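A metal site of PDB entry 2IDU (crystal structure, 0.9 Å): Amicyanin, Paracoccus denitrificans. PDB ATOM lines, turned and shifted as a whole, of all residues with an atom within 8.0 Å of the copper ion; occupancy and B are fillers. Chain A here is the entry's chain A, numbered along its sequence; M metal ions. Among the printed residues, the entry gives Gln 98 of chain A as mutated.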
ATOM      1  N   ILE A  25       1.333   1.703 -10.473  1.00  0.00           N
ATOM      2  CA  ILE A  25       1.022   3.089 -10.071  1.00  0.00           C
ATOM      3  C   ILE A  25       1.484   3.998 -11.193  1.00  0.00           C
ATOM      4  O   ILE A  25       2.684   4.102 -11.463  1.00  0.00           O
ATOM      5  CB  ILE A  25       1.651   3.441  -8.708  1.00  0.00           C
ATOM      6  CG1 ILE A  25       1.485   2.349  -7.664  1.00  0.00           C
ATOM      7  CG2 ILE A  25       1.057   4.752  -8.244  1.00  0.00           C
ATOM      8  CD1 ILE A  25       2.215   2.586  -6.367  1.00  0.00           C
ATOM      9  N   MET A  28      -0.830   8.914 -11.613  1.00  0.00           N
ATOM     10  CA  MET A  28      -1.195   9.383 -10.261  1.00  0.00           C
ATOM     11  C   MET A  28      -2.354   8.554  -9.702  1.00  0.00           C
ATOM     12  O   MET A  28      -3.154   9.069  -8.925  1.00  0.00           O
ATOM     13  CB  MET A  28      -1.484  10.882 -10.079  1.00  0.00           C
ATOM     14  CG  MET A  28      -0.250  11.747 -10.065  1.00  0.00           C
ATOM     15  SD  MET A  28       0.974  11.861  -8.773  1.00  0.00           S
ATOM     16  CE  MET A  28       0.048  12.476  -7.367  1.00  0.00           C
ATOM     17  N   LYS A  29      -2.448   7.278 -10.082  1.00  0.00           N
ATOM     18  CA  LYS A  29      -3.500   6.393  -9.583  1.00  0.00           C
ATOM     19  C   LYS A  29      -2.955   4.984  -9.418  1.00  0.00           C
ATOM     20  O   LYS A  29      -2.000   4.576 -10.062  1.00  0.00           O
ATOM     21  CB  LYS A  29      -4.697   6.353 -10.510  1.00  0.00           C
ATOM     22  CG  LYS A  29      -5.320   7.673 -10.785  1.00  0.00           C
ATOM     23  CD  LYS A  29      -6.257   7.658 -12.011  1.00  0.00           C
ATOM     24  CE  LYS A  29      -6.248   9.066 -12.629  1.00  0.00           C
ATOM     25  NZ  LYS A  29      -7.169   9.149 -13.808  1.00  0.00           N
ATOM     26  N   TYR A  30      -3.596   4.236  -8.529  1.00  0.00           N
ATOM     27  CA  TYR A  30      -3.433   2.784  -8.510  1.00  0.00           C
ATOM     28  C   TYR A  30      -4.248   2.249  -9.699  1.00  0.00           C
ATOM     29  O   TYR A  30      -5.468   2.417  -9.751  1.00  0.00           O
ATOM     30  CB  TYR A  30      -3.929   2.205  -7.208  1.00  0.00           C
ATOM     31  CG  TYR A  30      -3.196   2.722  -5.989  1.00  0.00           C
ATOM     32  CD1 TYR A  30      -1.878   2.427  -5.727  1.00  0.00           C
ATOM     33  CD2 TYR A  30      -3.872   3.493  -5.035  1.00  0.00           C
ATOM     34  CE1 TYR A  30      -1.220   2.912  -4.590  1.00  0.00           C
ATOM     35  CE2 TYR A  30      -3.260   3.964  -3.906  1.00  0.00           C
ATOM     36  CZ  TYR A  30      -1.933   3.674  -3.679  1.00  0.00           C
ATOM     37  OH  TYR A  30      -1.386   4.116  -2.499  1.00  0.00           O
ATOM     38  N   ASN A  47       5.793   1.421  -8.778  1.00  0.00           N
ATOM     39  CA  ASN A  47       5.676   2.840  -9.133  1.00  0.00           C
ATOM     40  C   ASN A  47       6.304   3.034 -10.527  1.00  0.00           C
ATOM     41  O   ASN A  47       7.490   2.823 -10.688  1.00  0.00           O
ATOM     42  CB  ASN A  47       6.350   3.709  -8.090  1.00  0.00           C
ATOM     43  CG  ASN A  47       6.146   5.188  -8.391  1.00  0.00           C
ATOM     44  OD1 ASN A  47       5.355   5.511  -9.317  1.00  0.00           O
ATOM     45  ND2 ASN A  47       6.810   6.055  -7.690  1.00  0.00           N
ATOM     46  N   GLU A  49       6.163   6.088 -12.123  1.00  0.00           N
ATOM     47  CA  GLU A  49       6.404   7.508 -12.412  1.00  0.00           C
ATOM     48  C   GLU A  49       7.373   8.155 -11.427  1.00  0.00           C
ATOM     49  O   GLU A  49       7.856   7.614 -10.430  1.00  0.00           O
ATOM     50  CB  GLU A  49       5.077   8.183 -12.700  1.00  0.00           C
ATOM     51  CG  GLU A  49       4.233   8.105 -11.522  1.00  0.00           C
ATOM     52  CD  GLU A  49       2.839   8.758 -11.645  1.00  0.00           C
ATOM     53  OE1 GLU A  49       2.301   9.139 -12.676  1.00  0.00           O
ATOM     54  OE2 GLU A  49       2.240   8.932 -10.586  1.00  0.00           O
ATOM     55  N   MHO A  51       7.097  10.848  -9.521  1.00  0.00           N
ATOM     56  CA  MHO A  51       6.607  11.189  -8.209  1.00  0.00           C
ATOM     57  CB  MHO A  51       5.167  11.719  -8.335  1.00  0.00           C
ATOM     58  CG  MHO A  51       4.549  12.054  -7.007  1.00  0.00           C
ATOM     59  SD  MHO A  51       5.388  13.283  -6.019  1.00  0.00           S
ATOM     60  CE  MHO A  51       5.088  14.755  -6.989  1.00  0.00           C
ATOM     61  C   MHO A  51       6.622   9.953  -7.333  1.00  0.00           C
ATOM     62  O   MHO A  51       6.066   8.935  -7.715  1.00  0.00           O
ATOM     63  OD1 MHO A  51       4.445  13.563  -4.792  1.00  0.00           O
ATOM     64  N   PRO A  52       7.180   9.989  -6.143  1.00  0.00           N
ATOM     65  CA  PRO A  52       7.106   8.826  -5.194  1.00  0.00           C
ATOM     66  C   PRO A  52       5.671   8.521  -4.768  1.00  0.00           C
ATOM     67  O   PRO A  52       4.858   9.413  -4.652  1.00  0.00           O
ATOM     68  CB  PRO A  52       7.991   9.233  -4.040  1.00  0.00           C
ATOM     69  CG  PRO A  52       8.965  10.228  -4.666  1.00  0.00           C
ATOM     70  CD  PRO A  52       8.069  11.049  -5.564  1.00  0.00           C
ATOM     71  N   HIS A  53       5.460   7.262  -4.470  1.00  0.00           N
ATOM     72  CA  HIS A  53       4.192   6.764  -3.946  1.00  0.00           C
ATOM     73  C   HIS A  53       4.429   5.613  -2.956  1.00  0.00           C
ATOM     74  O   HIS A  53       5.466   4.980  -2.988  1.00  0.00           O
ATOM     75  CB  HIS A  53       3.338   6.171  -5.082  1.00  0.00           C
ATOM     76  CG  HIS A  53       2.907   7.143  -6.149  1.00  0.00           C
ATOM     77  ND1 HIS A  53       1.923   8.059  -5.996  1.00  0.00           N
ATOM     78  CD2 HIS A  53       3.363   7.270  -7.430  1.00  0.00           C
ATOM     79  CE1 HIS A  53       1.830   8.738  -7.133  1.00  0.00           C
ATOM     80  NE2 HIS A  53       2.654   8.264  -8.039  1.00  0.00           N
ATOM     81  N   ASN A  54       3.446   5.349  -2.115  1.00  0.00           N
ATOM     82  CA  ASN A  54       3.504   4.206  -1.238  1.00  0.00           C
ATOM     83  C   ASN A  54       2.099   3.582  -1.192  1.00  0.00           C
ATOM     84  O   ASN A  54       1.214   3.950  -1.975  1.00  0.00           O
ATOM     85  CB  ASN A  54       4.017   4.511   0.179  1.00  0.00           C
ATOM     86  CG  ASN A  54       3.034   5.282   1.025  1.00  0.00           C
ATOM     87  OD1 ASN A  54       2.111   5.873   0.491  1.00  0.00           O
ATOM     88  ND2 ASN A  54       3.238   5.249   2.322  1.00  0.00           N
ATOM     89  N   VAL A  55       1.922   2.634  -0.274  1.00  0.00           N
ATOM     90  CA  VAL A  55       0.614   2.133   0.143  1.00  0.00           C
ATOM     91  C   VAL A  55       0.546   2.260   1.664  1.00  0.00           C
ATOM     92  O   VAL A  55       1.514   1.974   2.348  1.00  0.00           O
ATOM     93  CB  VAL A  55       0.304   0.698  -0.324  1.00  0.00           C
ATOM     94  CG1 VAL A  55       0.229   0.671  -1.842  1.00  0.00           C
ATOM     95  CG2 VAL A  55       1.338  -0.320   0.185  1.00  0.00           C
ATOM     96  N   MET A  71       8.263   4.670   0.817  1.00  0.00           N
ATOM     97  CA  MET A  71       8.127   5.370  -0.452  1.00  0.00           C
ATOM     98  C   MET A  71       8.878   4.672  -1.543  1.00  0.00           C
ATOM     99  O   MET A  71      10.076   4.394  -1.439  1.00  0.00           O
ATOM    100  CB  MET A  71       8.583   6.836  -0.314  1.00  0.00           C
ATOM    101  CG  MET A  71       7.813   7.595   0.724  1.00  0.00           C
ATOM    102  SD  MET A  71       6.029   7.589   0.615  1.00  0.00           S
ATOM    103  CE  MET A  71       5.742   8.378  -0.939  1.00  0.00           C
ATOM    104  N   HIS A  91      -4.423   3.883   0.985  1.00  0.00           N
ATOM    105  CA  HIS A  91      -4.239   5.118   0.259  1.00  0.00           C
ATOM    106  C   HIS A  91      -2.765   5.409   0.142  1.00  0.00           C
ATOM    107  O   HIS A  91      -1.917   4.715   0.748  1.00  0.00           O
ATOM    108  CB  HIS A  91      -4.969   6.282   0.963  1.00  0.00           C
ATOM    109  CG  HIS A  91      -4.394   6.702   2.268  1.00  0.00           C
ATOM    110  ND1 HIS A  91      -4.649   6.049   3.424  1.00  0.00           N
ATOM    111  CD2 HIS A  91      -3.511   7.700   2.559  1.00  0.00           C
ATOM    112  CE1 HIS A  91      -3.975   6.635   4.440  1.00  0.00           C
ATOM    113  NE2 HIS A  91      -3.293   7.630   3.914  1.00  0.00           N
ATOM    114  N   CYS A  92      -2.414   6.444  -0.601  1.00  0.00           N
ATOM    115  CA  CYS A  92      -1.040   6.886  -0.744  1.00  0.00           C
ATOM    116  C   CYS A  92      -0.767   7.988   0.291  1.00  0.00           C
ATOM    117  O   CYS A  92      -1.486   8.997   0.307  1.00  0.00           O
ATOM    118  CB  CYS A  92      -0.841   7.379  -2.176  1.00  0.00           C
ATOM    119  SG  CYS A  92       0.893   7.774  -2.421  1.00  0.00           S
ATOM    120  N   THR A  93       0.214   7.817   1.154  1.00  0.00           N
ATOM    121  CA  THR A  93       0.440   8.772   2.233  1.00  0.00           C
ATOM    122  C   THR A  93       0.559  10.218   1.731  1.00  0.00           C
ATOM    123  O   THR A  93      -0.147  11.107   2.213  1.00  0.00           O
ATOM    124  CB  THR A  93       1.652   8.378   3.083  1.00  0.00           C
ATOM    125  OG1 THR A  93       1.461   7.055   3.570  1.00  0.00           O
ATOM    126  CG2 THR A  93       1.851   9.340   4.249  1.00  0.00           C
ATOM    127  N   PRO A  94       1.447  10.495   0.749  1.00  0.00           N
ATOM    128  CA  PRO A  94       1.584  11.880   0.299  1.00  0.00           C
ATOM    129  C   PRO A  94       0.385  12.368  -0.523  1.00  0.00           C
ATOM    130  O   PRO A  94       0.274  13.572  -0.745  1.00  0.00           O
ATOM    131  CB  PRO A  94       2.835  11.872  -0.571  1.00  0.00           C
ATOM    132  CG  PRO A  94       2.901  10.488  -1.093  1.00  0.00           C
ATOM    133  CD  PRO A  94       2.493   9.648   0.138  1.00  0.00           C
ATOM    134  N   HIS A  95      -0.444  11.447  -1.032  1.00  0.00           N
ATOM    135  CA  HIS A  95      -1.543  11.750  -1.935  1.00  0.00           C
ATOM    136  C   HIS A  95      -2.822  11.077  -1.473  1.00  0.00           C
ATOM    137  O   HIS A  95      -3.263  10.057  -2.024  1.00  0.00           O
ATOM    138  CB  HIS A  95      -1.247  11.270  -3.344  1.00  0.00           C
ATOM    139  CG  HIS A  95       0.094  11.675  -3.817  1.00  0.00           C
ATOM    140  ND1 HIS A  95       0.984  10.750  -4.295  1.00  0.00           N
ATOM    141  CD2 HIS A  95       0.680  12.889  -3.969  1.00  0.00           C
ATOM    142  CE1 HIS A  95       2.067  11.348  -4.649  1.00  0.00           C
ATOM    143  NE2 HIS A  95       1.923  12.628  -4.474  1.00  0.00           N
ATOM    144  N   PRO A  96      -3.448  11.551  -0.385  1.00  0.00           N
ATOM    145  CA  PRO A  96      -4.538  10.800   0.205  1.00  0.00           C
ATOM    146  C   PRO A  96      -5.758  10.660  -0.685  1.00  0.00           C
ATOM    147  O   PRO A  96      -6.609   9.780  -0.435  1.00  0.00           O
ATOM    148  CB  PRO A  96      -4.813  11.522   1.531  1.00  0.00           C
ATOM    149  CG  PRO A  96      -4.269  12.909   1.305  1.00  0.00           C
ATOM    150  CD  PRO A  96      -3.019  12.673   0.457  1.00  0.00           C
ATOM    151  N   PHE A  97      -5.890  11.513  -1.719  1.00  0.00           N
ATOM    152  CA  PHE A  97      -6.907  11.318  -2.739  1.00  0.00           C
ATOM    153  C   PHE A  97      -6.747  10.066  -3.572  1.00  0.00           C
ATOM    154  O   PHE A  97      -7.677   9.689  -4.253  1.00  0.00           O
ATOM    155  CB  PHE A  97      -6.939  12.562  -3.677  1.00  0.00           C
ATOM    156  CG  PHE A  97      -5.586  13.022  -4.103  1.00  0.00           C
ATOM    157  CD1 PHE A  97      -5.024  12.447  -5.227  1.00  0.00           C
ATOM    158  CD2 PHE A  97      -4.838  13.989  -3.422  1.00  0.00           C
ATOM    159  CE1 PHE A  97      -3.785  12.800  -5.721  1.00  0.00           C
ATOM    160  CE2 PHE A  97      -3.581  14.346  -3.899  1.00  0.00           C
ATOM    161  CZ  PHE A  97      -3.102  13.764  -5.037  1.00  0.00           C
ATOM    162  N   GLN A  98      -5.609   9.410  -3.504  1.00  0.00           N
ATOM    163  CA  GLN A  98      -5.281   8.219  -4.269  1.00  0.00           C
ATOM    164  C   GLN A  98      -5.532   6.986  -3.394  1.00  0.00           C
ATOM    165  O   GLN A  98      -4.825   6.779  -2.426  1.00  0.00           O
ATOM    166  CB  GLN A  98      -3.827   8.070  -4.696  1.00  0.00           C
ATOM    167  CG  GLN A  98      -3.443   8.820  -5.943  1.00  0.00           C
ATOM    168  CD  GLN A  98      -1.964   8.725  -6.293  1.00  0.00           C
ATOM    169  OE1 GLN A  98      -1.192   7.852  -5.955  1.00  0.00           O
ATOM    170  NE2 GLN A  98      -1.611   9.746  -7.065  1.00  0.00           N
ATOM    171  N   ARG A  99      -6.612   6.255  -3.700  1.00  0.00           N
ATOM    172  CA  ARG A  99      -7.118   5.194  -2.878  1.00  0.00           C
ATOM    173  C   ARG A  99      -7.260   3.864  -3.665  1.00  0.00           C
ATOM    174  O   ARG A  99      -7.449   3.901  -4.882  1.00  0.00           O
ATOM    175  CB  ARG A  99      -8.482   5.568  -2.292  1.00  0.00           C
ATOM    176  CG  ARG A  99      -8.470   6.849  -1.521  1.00  0.00           C
ATOM    177  CD  ARG A  99      -8.898   6.831  -0.177  1.00  0.00           C
ATOM    178  NE  ARG A  99      -8.447   7.980   0.571  1.00  0.00           N
ATOM    179  CZ  ARG A  99      -8.245   7.961   1.896  1.00  0.00           C
ATOM    180  NH1 ARG A  99      -8.433   6.872   2.652  1.00  0.00           N
ATOM    181  NH2 ARG A  99      -7.812   9.070   2.480  1.00  0.00           N
HETATM  182 CU    CU M   1       0.767   8.706  -4.437  1.00  0.00          CU
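Of the 21 residues printed, 4 come within 4 Å of the copper ion.
The nearest printed residue that does not touch the copper ion is Pro 52 (4.2 Å).
OE1 of Gln 98 lies close to ND1 of His 53, at 3.1 Å.
A ring nitrogen (NE2) of His 53 sits close to O of MHO 51 (3.5 Å).
The side-chain carboxylate (OE2) of Glu 49 is in hydrogen-bond range of a ring nitrogen (NE2) of His 53 (2.7 Å).
NE2 of His 95 sits at hydrogen-bond distance from OD1 of MHO 51.
The backbone carbonyl oxygen of Gln 98 sits at hydrogen-bond distance from the backbone NH of Cys 92.
SG of Cys 92 lies close to N of Asn 54, at 3.5 Å.
The backbone NH (N) of Cys 92 lies within hydrogen-bond range of the side-chain hydroxyl (OH) of Tyr 30.
The backbone carbonyl oxygen (O) of Met 28 is in hydrogen-bond range of the side-chain amide nitrogen (NE2) of Gln 98, at 2.5 Å.
The copper ion is bound by ND1 of His 53 (2.0 Å), ND1 of His 95 (2.1 Å) and SG of Cys 92 (2.2 Å).
The copper ion has three donor atoms within binding distance.
Slightly farther from the copper ion lies the side-chain amide oxygen (OE1) of Gln 98 (2.6 Å).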
